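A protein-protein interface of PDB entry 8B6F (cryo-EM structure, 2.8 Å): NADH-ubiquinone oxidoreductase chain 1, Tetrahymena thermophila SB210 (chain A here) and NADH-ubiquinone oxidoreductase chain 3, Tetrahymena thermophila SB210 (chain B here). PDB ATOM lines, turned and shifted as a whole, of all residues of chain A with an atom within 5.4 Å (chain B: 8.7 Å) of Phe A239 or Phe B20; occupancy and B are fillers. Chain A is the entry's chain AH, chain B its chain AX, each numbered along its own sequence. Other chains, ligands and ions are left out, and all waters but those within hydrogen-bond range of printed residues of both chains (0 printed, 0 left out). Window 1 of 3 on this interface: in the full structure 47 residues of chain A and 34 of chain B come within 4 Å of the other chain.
Of chain B, only Phe B20 comes within 4 Å of Phe A239. Phe B20 touches just these residues of chain A: Phe A75 (3.5 Å), Tyr A102 (3.4 Å) and Phe A239 (3.3 Å). No residue of chain B comes within 4 Å of Gly A238. Printed residues of chain B within 4 Å of Phe A75: Phe B20 (3.5 Å), Leu B23 (3.6 Å), Thr B24 (3.99 Å) and Ala B27 (3.3 Å). Of the printed residues of chain B, Tyr A102 touches Val B13, Phe B16 and Phe B20. Printed residues of chain A within 4 Å of Leu B23: Phe A75 (3.6 Å). Of the printed residues of chain A, Thr B24 touches Phe A75 (3.99 Å). Of the printed residues of chain A, Phe B16 touches Tyr A102 (3.3 Å). The nearest residue of chain B that does not touch Phe A239 is Thr B24 (4.2 Å).
OH of Tyr A102 lies within hydrogen-bond range of OG1 of Thr A33, 2.8 Å away. N of Phe A239 is in hydrogen-bond range of O of Leu A74, 3.4 Å away. The backbone carbonyl oxygen of Phe B20 lies within hydrogen-bond range of the side-chain hydroxyl of Thr B24.
Among the printed residues, pairs that only touch across the chains: Phe A75 with Phe B20 (3.5 Å), Phe A75 with Leu B23 (3.6 Å), Phe A75 with Thr B24 (3.99 Å), Phe A75 with Ala B27 (3.3 Å), Tyr A102 with Val B13 (3.96 Å), Tyr A102 with Phe B16 (3.3 Å), Tyr A102 with Phe B20 (3.4 Å) and Phe A239 with Phe B20 (3.3 Å).
Hydrophobic or aromatic side chains of chain A within 4 Å of the printed part of chain B: Phe A75, Tyr A102 and Phe A239. Along chain A the printed residues that touch a printed residue of chain B span positions 75 to 239. Printed residues of chain B that touch a printed residue of chain A: Val B13, Phe B16, Phe B20, Leu B23, Thr B24 and Ala B27.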
ATOM      1  N   THR A  33      17.566  13.387  16.705  1.00  0.00           N
ATOM      2  CA  THR A  33      17.853  14.717  17.234  1.00  0.00           C
ATOM      3  C   THR A  33      18.885  14.645  18.351  1.00  0.00           C
ATOM      4  O   THR A  33      19.798  15.476  18.417  1.00  0.00           O
ATOM      5  CB  THR A  33      16.570  15.374  17.745  1.00  0.00           C
ATOM      6  OG1 THR A  33      15.604  15.435  16.691  1.00  0.00           O
ATOM      7  CG2 THR A  33      16.849  16.784  18.249  1.00  0.00           C
ATOM      8  N   LEU A  74      17.682  27.982  23.071  1.00  0.00           N
ATOM      9  CA  LEU A  74      17.164  28.364  21.761  1.00  0.00           C
ATOM     10  C   LEU A  74      15.641  28.335  21.747  1.00  0.00           C
ATOM     11  O   LEU A  74      15.003  29.199  21.137  1.00  0.00           O
ATOM     12  CB  LEU A  74      17.743  27.443  20.686  1.00  0.00           C
ATOM     13  CG  LEU A  74      19.238  27.633  20.397  1.00  0.00           C
ATOM     14  CD1 LEU A  74      19.759  26.577  19.436  1.00  0.00           C
ATOM     15  CD2 LEU A  74      19.516  29.023  19.839  1.00  0.00           C
ATOM     16  N   PHE A  75      15.040  27.347  22.411  1.00  0.00           N
ATOM     17  CA  PHE A  75      13.591  27.355  22.579  1.00  0.00           C
ATOM     18  C   PHE A  75      13.138  28.608  23.318  1.00  0.00           C
ATOM     19  O   PHE A  75      12.160  29.254  22.924  1.00  0.00           O
ATOM     20  CB  PHE A  75      13.138  26.108  23.341  1.00  0.00           C
ATOM     21  CG  PHE A  75      12.956  24.897  22.476  1.00  0.00           C
ATOM     22  CD1 PHE A  75      11.950  24.850  21.528  1.00  0.00           C
ATOM     23  CD2 PHE A  75      13.773  23.792  22.635  1.00  0.00           C
ATOM     24  CE1 PHE A  75      11.777  23.734  20.739  1.00  0.00           C
ATOM     25  CE2 PHE A  75      13.605  22.672  21.851  1.00  0.00           C
ATOM     26  CZ  PHE A  75      12.604  22.642  20.902  1.00  0.00           C
ATOM     27  N   LYS A  77      14.509  31.595  23.744  1.00  0.00           N
ATOM     28  CA  LYS A  77      14.742  32.904  23.147  1.00  0.00           C
ATOM     29  C   LYS A  77      13.524  33.362  22.354  1.00  0.00           C
ATOM     30  O   LYS A  77      12.951  32.595  21.576  1.00  0.00           O
ATOM     31  CB  LYS A  77      15.979  32.850  22.249  1.00  0.00           C
ATOM     32  CG  LYS A  77      16.313  34.158  21.540  1.00  0.00           C
ATOM     33  CD  LYS A  77      16.656  35.277  22.516  1.00  0.00           C
ATOM     34  CE  LYS A  77      17.966  35.028  23.242  1.00  0.00           C
ATOM     35  NZ  LYS A  77      19.111  34.903  22.300  1.00  0.00           N
ATOM     36  N   ILE A  79      11.351  35.685  19.555  1.00  0.00           N
ATOM     37  CA  ILE A  79      11.528  35.950  18.131  1.00  0.00           C
ATOM     38  C   ILE A  79      10.604  37.088  17.721  1.00  0.00           C
ATOM     39  O   ILE A  79       9.469  37.184  18.200  1.00  0.00           O
ATOM     40  CB  ILE A  79      11.246  34.697  17.273  1.00  0.00           C
ATOM     41  CG1 ILE A  79      12.125  33.528  17.729  1.00  0.00           C
ATOM     42  CG2 ILE A  79      11.488  35.000  15.799  1.00  0.00           C
ATOM     43  CD1 ILE A  79      11.796  32.208  17.057  1.00  0.00           C
ATOM     44  N   TYR A 102      14.122  16.914   8.996  1.00  0.00           N
ATOM     45  CA  TYR A 102      13.646  15.779   9.772  1.00  0.00           C
ATOM     46  C   TYR A 102      13.089  14.664   8.904  1.00  0.00           C
ATOM     47  O   TYR A 102      12.797  13.585   9.426  1.00  0.00           O
ATOM     48  CB  TYR A 102      12.592  16.229  10.782  1.00  0.00           C
ATOM     49  CG  TYR A 102      13.200  16.681  12.085  1.00  0.00           C
ATOM     50  CD1 TYR A 102      13.616  15.753  13.028  1.00  0.00           C
ATOM     51  CD2 TYR A 102      13.372  18.028  12.369  1.00  0.00           C
ATOM     52  CE1 TYR A 102      14.179  16.150  14.218  1.00  0.00           C
ATOM     53  CE2 TYR A 102      13.936  18.438  13.561  1.00  0.00           C
ATOM     54  CZ  TYR A 102      14.339  17.492  14.480  1.00  0.00           C
ATOM     55  OH  TYR A 102      14.900  17.891  15.670  1.00  0.00           O
ATOM     56  N   GLY A 237      16.622  34.245  14.695  1.00  0.00           N
ATOM     57  CA  GLY A 237      17.077  33.855  16.008  1.00  0.00           C
ATOM     58  C   GLY A 237      16.141  32.824  16.613  1.00  0.00           C
ATOM     59  O   GLY A 237      15.094  32.496  16.051  1.00  0.00           O
ATOM     60  N   GLY A 238      16.543  32.314  17.773  1.00  0.00           N
ATOM     61  CA  GLY A 238      15.725  31.329  18.449  1.00  0.00           C
ATOM     62  C   GLY A 238      15.630  30.032  17.666  1.00  0.00           C
ATOM     63  O   GLY A 238      16.565  29.616  16.975  1.00  0.00           O
ATOM     64  N   PHE A 239      14.471  29.379  17.773  1.00  0.00           N
ATOM     65  CA  PHE A 239      14.320  28.064  17.164  1.00  0.00           C
ATOM     66  C   PHE A 239      14.278  28.123  15.644  1.00  0.00           C
ATOM     67  O   PHE A 239      14.514  27.099  14.994  1.00  0.00           O
ATOM     68  CB  PHE A 239      13.073  27.362  17.696  1.00  0.00           C
ATOM     69  CG  PHE A 239      13.107  25.875  17.506  1.00  0.00           C
ATOM     70  CD1 PHE A 239      13.922  25.084  18.298  1.00  0.00           C
ATOM     71  CD2 PHE A 239      12.337  25.269  16.531  1.00  0.00           C
ATOM     72  CE1 PHE A 239      13.964  23.717  18.122  1.00  0.00           C
ATOM     73  CE2 PHE A 239      12.374  23.902  16.350  1.00  0.00           C
ATOM     74  CZ  PHE A 239      13.188  23.124  17.147  1.00  0.00           C
ATOM     75  N   TYR A 240      13.979  29.283  15.060  1.00  0.00           N
ATOM     76  CA  TYR A 240      14.064  29.412  13.609  1.00  0.00           C
ATOM     77  C   TYR A 240      15.485  29.145  13.130  1.00  0.00           C
ATOM     78  O   TYR A 240      15.694  28.426  12.148  1.00  0.00           O
ATOM     79  CB  TYR A 240      13.605  30.801  13.166  1.00  0.00           C
ATOM     80  CG  TYR A 240      12.137  31.091  13.397  1.00  0.00           C
ATOM     81  CD1 TYR A 240      11.272  30.113  13.873  1.00  0.00           C
ATOM     82  CD2 TYR A 240      11.614  32.346  13.122  1.00  0.00           C
ATOM     83  CE1 TYR A 240       9.934  30.382  14.076  1.00  0.00           C
ATOM     84  CE2 TYR A 240      10.279  32.623  13.322  1.00  0.00           C
ATOM     85  CZ  TYR A 240       9.445  31.639  13.799  1.00  0.00           C
ATOM     86  OH  TYR A 240       8.113  31.916  13.997  1.00  0.00           O
ATOM     87  N   PHE A 241      16.473  29.713  13.820  1.00  0.00           N
ATOM     88  CA  PHE A 241      17.869  29.429  13.507  1.00  0.00           C
ATOM     89  C   PHE A 241      18.285  28.048  13.994  1.00  0.00           C
ATOM     90  O   PHE A 241      19.122  27.397  13.359  1.00  0.00           O
ATOM     91  CB  PHE A 241      18.764  30.509  14.113  1.00  0.00           C
ATOM     92  CG  PHE A 241      20.172  30.059  14.370  1.00  0.00           C
ATOM     93  CD1 PHE A 241      21.093  29.981  13.339  1.00  0.00           C
ATOM     94  CD2 PHE A 241      20.582  29.744  15.654  1.00  0.00           C
ATOM     95  CE1 PHE A 241      22.390  29.577  13.580  1.00  0.00           C
ATOM     96  CE2 PHE A 241      21.878  29.339  15.902  1.00  0.00           C
ATOM     97  CZ  PHE A 241      22.783  29.258  14.864  1.00  0.00           C
ATOM     98  N   ALA A 242      17.715  27.579  15.103  1.00  0.00           N
ATOM     99  CA  ALA A 242      18.009  26.226  15.564  1.00  0.00           C
ATOM    100  C   ALA A 242      17.642  25.198  14.506  1.00  0.00           C
ATOM    101  O   ALA A 242      18.346  24.196  14.331  1.00  0.00           O
ATOM    102  CB  ALA A 242      17.250  25.932  16.855  1.00  0.00           C
ATOM    103  N   LEU A 243      16.544  25.428  13.786  1.00  0.00           N
ATOM    104  CA  LEU A 243      16.135  24.494  12.742  1.00  0.00           C
ATOM    105  C   LEU A 243      17.173  24.418  11.633  1.00  0.00           C
ATOM    106  O   LEU A 243      17.495  23.327  11.151  1.00  0.00           O
ATOM    107  CB  LEU A 243      14.774  24.899  12.179  1.00  0.00           C
ATOM    108  CG  LEU A 243      13.561  24.620  13.070  1.00  0.00           C
ATOM    109  CD1 LEU A 243      12.307  25.234  12.480  1.00  0.00           C
ATOM    110  CD2 LEU A 243      13.371  23.123  13.267  1.00  0.00           C
ATOM    111  N   TYR A 244      17.706  25.562  11.207  1.00  0.00           N
ATOM    112  CA  TYR A 244      18.740  25.542  10.178  1.00  0.00           C
ATOM    113  C   TYR A 244      19.989  24.822  10.670  1.00  0.00           C
ATOM    114  O   TYR A 244      20.594  24.038   9.930  1.00  0.00           O
ATOM    115  CB  TYR A 244      19.077  26.968   9.750  1.00  0.00           C
ATOM    116  CG  TYR A 244      17.950  27.664   9.028  1.00  0.00           C
ATOM    117  CD1 TYR A 244      17.623  27.326   7.723  1.00  0.00           C
ATOM    118  CD2 TYR A 244      17.219  28.665   9.650  1.00  0.00           C
ATOM    119  CE1 TYR A 244      16.597  27.961   7.059  1.00  0.00           C
ATOM    120  CE2 TYR A 244      16.191  29.307   8.994  1.00  0.00           C
ATOM    121  CZ  TYR A 244      15.884  28.951   7.700  1.00  0.00           C
ATOM    122  OH  TYR A 244      14.860  29.588   7.041  1.00  0.00           O
ATOM    123  N   LEU A 246      20.142  22.466  12.968  1.00  0.00           N
ATOM    124  CA  LEU A 246      19.827  21.043  13.020  1.00  0.00           C
ATOM    125  C   LEU A 246      19.860  20.423  11.632  1.00  0.00           C
ATOM    126  O   LEU A 246      20.360  19.306  11.454  1.00  0.00           O
ATOM    127  CB  LEU A 246      18.456  20.830  13.665  1.00  0.00           C
ATOM    128  CG  LEU A 246      18.348  21.092  15.168  1.00  0.00           C
ATOM    129  CD1 LEU A 246      16.907  20.972  15.620  1.00  0.00           C
ATOM    130  CD2 LEU A 246      19.229  20.136  15.957  1.00  0.00           C
ATOM    131  N   VAL B  13       6.034  13.834  10.317  1.00  0.00           N
ATOM    132  CA  VAL B  13       7.053  14.856  10.538  1.00  0.00           C
ATOM    133  C   VAL B  13       6.404  16.193  10.871  1.00  0.00           C
ATOM    134  O   VAL B  13       6.897  16.939  11.726  1.00  0.00           O
ATOM    135  CB  VAL B  13       7.979  14.963   9.313  1.00  0.00           C
ATOM    136  CG1 VAL B  13       8.857  16.208   9.402  1.00  0.00           C
ATOM    137  CG2 VAL B  13       8.850  13.727   9.203  1.00  0.00           C
ATOM    138  N   LEU B  14       5.296  16.522  10.207  1.00  0.00           N
ATOM    139  CA  LEU B  14       4.570  17.735  10.564  1.00  0.00           C
ATOM    140  C   LEU B  14       4.048  17.659  11.993  1.00  0.00           C
ATOM    141  O   LEU B  14       4.135  18.635  12.746  1.00  0.00           O
ATOM    142  CB  LEU B  14       3.426  17.967   9.578  1.00  0.00           C
ATOM    143  CG  LEU B  14       3.824  18.146   8.110  1.00  0.00           C
ATOM    144  CD1 LEU B  14       2.598  18.451   7.268  1.00  0.00           C
ATOM    145  CD2 LEU B  14       4.882  19.227   7.937  1.00  0.00           C
ATOM    146  N   ILE B  15       3.501  16.509  12.387  1.00  0.00           N
ATOM    147  CA  ILE B  15       3.031  16.342  13.759  1.00  0.00           C
ATOM    148  C   ILE B  15       4.190  16.496  14.736  1.00  0.00           C
ATOM    149  O   ILE B  15       4.034  17.046  15.830  1.00  0.00           O
ATOM    150  CB  ILE B  15       2.322  14.987  13.931  1.00  0.00           C
ATOM    151  CG1 ILE B  15       1.061  14.913  13.061  1.00  0.00           C
ATOM    152  CG2 ILE B  15       1.966  14.758  15.395  1.00  0.00           C
ATOM    153  CD1 ILE B  15      -0.014  15.928  13.403  1.00  0.00           C
ATOM    154  N   PHE B  16       5.368  15.998  14.359  1.00  0.00           N
ATOM    155  CA  PHE B  16       6.549  16.165  15.198  1.00  0.00           C
ATOM    156  C   PHE B  16       6.907  17.637  15.346  1.00  0.00           C
ATOM    157  O   PHE B  16       7.205  18.103  16.452  1.00  0.00           O
ATOM    158  CB  PHE B  16       7.724  15.386  14.611  1.00  0.00           C
ATOM    159  CG  PHE B  16       8.997  15.536  15.389  1.00  0.00           C
ATOM    160  CD1 PHE B  16       9.156  14.898  16.608  1.00  0.00           C
ATOM    161  CD2 PHE B  16      10.039  16.303  14.899  1.00  0.00           C
ATOM    162  CE1 PHE B  16      10.326  15.028  17.327  1.00  0.00           C
ATOM    163  CE2 PHE B  16      11.210  16.437  15.615  1.00  0.00           C
ATOM    164  CZ  PHE B  16      11.355  15.799  16.830  1.00  0.00           C
ATOM    165  N   GLY B  17       6.880  18.386  14.246  1.00  0.00           N
ATOM    166  CA  GLY B  17       7.137  19.813  14.330  1.00  0.00           C
ATOM    167  C   GLY B  17       6.141  20.542  15.209  1.00  0.00           C
ATOM    168  O   GLY B  17       6.460  21.590  15.777  1.00  0.00           O
ATOM    169  N   ILE B  18       4.921  20.014  15.328  1.00  0.00           N
ATOM    170  CA  ILE B  18       3.956  20.597  16.258  1.00  0.00           C
ATOM    171  C   ILE B  18       4.482  20.537  17.686  1.00  0.00           C
ATOM    172  O   ILE B  18       4.137  21.385  18.516  1.00  0.00           O
ATOM    173  CB  ILE B  18       2.589  19.895  16.128  1.00  0.00           C
ATOM    174  CG1 ILE B  18       1.939  20.265  14.795  1.00  0.00           C
ATOM    175  CG2 ILE B  18       1.671  20.271  17.292  1.00  0.00           C
ATOM    176  CD1 ILE B  18       0.655  19.523  14.506  1.00  0.00           C
ATOM    177  N   ILE B  19       5.313  19.542  18.002  1.00  0.00           N
ATOM    178  CA  ILE B  19       5.884  19.460  19.343  1.00  0.00           C
ATOM    179  C   ILE B  19       6.809  20.643  19.592  1.00  0.00           C
ATOM    180  O   ILE B  19       6.750  21.288  20.645  1.00  0.00           O
ATOM    181  CB  ILE B  19       6.619  18.122  19.537  1.00  0.00           C
ATOM    182  CG1 ILE B  19       5.652  16.951  19.341  1.00  0.00           C
ATOM    183  CG2 ILE B  19       7.257  18.064  20.921  1.00  0.00           C
ATOM    184  CD1 ILE B  19       6.322  15.593  19.323  1.00  0.00           C
ATOM    185  N   PHE B  20       7.686  20.942  18.633  1.00  0.00           N
ATOM    186  CA  PHE B  20       8.540  22.115  18.764  1.00  0.00           C
ATOM    187  C   PHE B  20       7.717  23.394  18.795  1.00  0.00           C
ATOM    188  O   PHE B  20       8.084  24.352  19.484  1.00  0.00           O
ATOM    189  CB  PHE B  20       9.553  22.161  17.620  1.00  0.00           C
ATOM    190  CG  PHE B  20      10.552  21.035  17.641  1.00  0.00           C
ATOM    191  CD1 PHE B  20      10.906  20.415  18.830  1.00  0.00           C
ATOM    192  CD2 PHE B  20      11.138  20.599  16.466  1.00  0.00           C
ATOM    193  CE1 PHE B  20      11.825  19.385  18.845  1.00  0.00           C
ATOM    194  CE2 PHE B  20      12.058  19.569  16.474  1.00  0.00           C
ATOM    195  CZ  PHE B  20      12.401  18.962  17.667  1.00  0.00           C
ATOM    196  N   TRP B  21       6.609  23.432  18.055  1.00  0.00           N
ATOM    197  CA  TRP B  21       5.712  24.580  18.121  1.00  0.00           C
ATOM    198  C   TRP B  21       5.170  24.758  19.533  1.00  0.00           C
ATOM    199  O   TRP B  21       5.137  25.873  20.062  1.00  0.00           O
ATOM    200  CB  TRP B  21       4.574  24.404  17.114  1.00  0.00           C
ATOM    201  CG  TRP B  21       3.561  25.514  17.116  1.00  0.00           C
ATOM    202  CD1 TRP B  21       3.709  26.763  17.644  1.00  0.00           C
ATOM    203  CD2 TRP B  21       2.243  25.465  16.562  1.00  0.00           C
ATOM    204  NE1 TRP B  21       2.563  27.495  17.451  1.00  0.00           N
ATOM    205  CE2 TRP B  21       1.648  26.720  16.790  1.00  0.00           C
ATOM    206  CE3 TRP B  21       1.507  24.480  15.895  1.00  0.00           C
ATOM    207  CZ2 TRP B  21       0.353  27.018  16.375  1.00  0.00           C
ATOM    208  CZ3 TRP B  21       0.222  24.777  15.482  1.00  0.00           C
ATOM    209  CH2 TRP B  21      -0.342  26.037  15.722  1.00  0.00           C
ATOM    210  N   LEU B  22       4.741  23.662  20.162  1.00  0.00           N
ATOM    211  CA  LEU B  22       4.247  23.745  21.531  1.00  0.00           C
ATOM    212  C   LEU B  22       5.334  24.232  22.479  1.00  0.00           C
ATOM    213  O   LEU B  22       5.078  25.066  23.355  1.00  0.00           O
ATOM    214  CB  LEU B  22       3.725  22.381  21.982  1.00  0.00           C
ATOM    215  CG  LEU B  22       2.315  21.986  21.544  1.00  0.00           C
ATOM    216  CD1 LEU B  22       2.013  20.548  21.918  1.00  0.00           C
ATOM    217  CD2 LEU B  22       1.291  22.917  22.175  1.00  0.00           C
ATOM    218  N   LEU B  23       6.555  23.718  22.325  1.00  0.00           N
ATOM    219  CA  LEU B  23       7.647  24.153  23.189  1.00  0.00           C
ATOM    220  C   LEU B  23       7.933  25.636  23.000  1.00  0.00           C
ATOM    221  O   LEU B  23       8.155  26.364  23.974  1.00  0.00           O
ATOM    222  CB  LEU B  23       8.898  23.322  22.908  1.00  0.00           C
ATOM    223  CG  LEU B  23       8.839  21.855  23.342  1.00  0.00           C
ATOM    224  CD1 LEU B  23      10.068  21.107  22.859  1.00  0.00           C
ATOM    225  CD2 LEU B  23       8.702  21.732  24.850  1.00  0.00           C
ATOM    226  N   THR B  24       7.947  26.103  21.749  1.00  0.00           N
ATOM    227  CA  THR B  24       8.193  27.518  21.499  1.00  0.00           C
ATOM    228  C   THR B  24       7.100  28.384  22.113  1.00  0.00           C
ATOM    229  O   THR B  24       7.388  29.431  22.704  1.00  0.00           O
ATOM    230  CB  THR B  24       8.287  27.772  19.995  1.00  0.00           C
ATOM    231  OG1 THR B  24       9.233  26.869  19.411  1.00  0.00           O
ATOM    232  CG2 THR B  24       8.728  29.200  19.720  1.00  0.00           C
ATOM    233  N   TRP B  25       5.840  27.970  21.975  1.00  0.00           N
ATOM    234  CA  TRP B  25       4.745  28.729  22.571  1.00  0.00           C
ATOM    235  C   TRP B  25       4.861  28.759  24.088  1.00  0.00           C
ATOM    236  O   TRP B  25       4.698  29.811  24.715  1.00  0.00           O
ATOM    237  CB  TRP B  25       3.402  28.135  22.153  1.00  0.00           C
ATOM    238  CG  TRP B  25       2.240  28.863  22.745  1.00  0.00           C
ATOM    239  CD1 TRP B  25       2.113  30.212  22.897  1.00  0.00           C
ATOM    240  CD2 TRP B  25       1.044  28.284  23.278  1.00  0.00           C
ATOM    241  NE1 TRP B  25       0.910  30.510  23.486  1.00  0.00           N
ATOM    242  CE2 TRP B  25       0.234  29.344  23.729  1.00  0.00           C
ATOM    243  CE3 TRP B  25       0.578  26.974  23.413  1.00  0.00           C
ATOM    244  CZ2 TRP B  25      -1.014  29.134  24.307  1.00  0.00           C
ATOM    245  CZ3 TRP B  25      -0.662  26.767  23.986  1.00  0.00           C
ATOM    246  CH2 TRP B  25      -1.445  27.842  24.426  1.00  0.00           C
ATOM    247  N   GLY B  26       5.146  27.607  24.697  1.00  0.00           N
ATOM    248  CA  GLY B  26       5.292  27.565  26.142  1.00  0.00           C
ATOM    249  C   GLY B  26       6.425  28.436  26.638  1.00  0.00           C
ATOM    250  O   GLY B  26       6.332  29.030  27.714  1.00  0.00           O
ATOM    251  N   ALA B  27       7.504  28.529  25.862  1.00  0.00           N
ATOM    252  CA  ALA B  27       8.624  29.380  26.238  1.00  0.00           C
ATOM    253  C   ALA B  27       8.227  30.845  26.346  1.00  0.00           C
ATOM    254  O   ALA B  27       8.941  31.622  26.987  1.00  0.00           O
ATOM    255  CB  ALA B  27       9.753  29.226  25.226  1.00  0.00           C
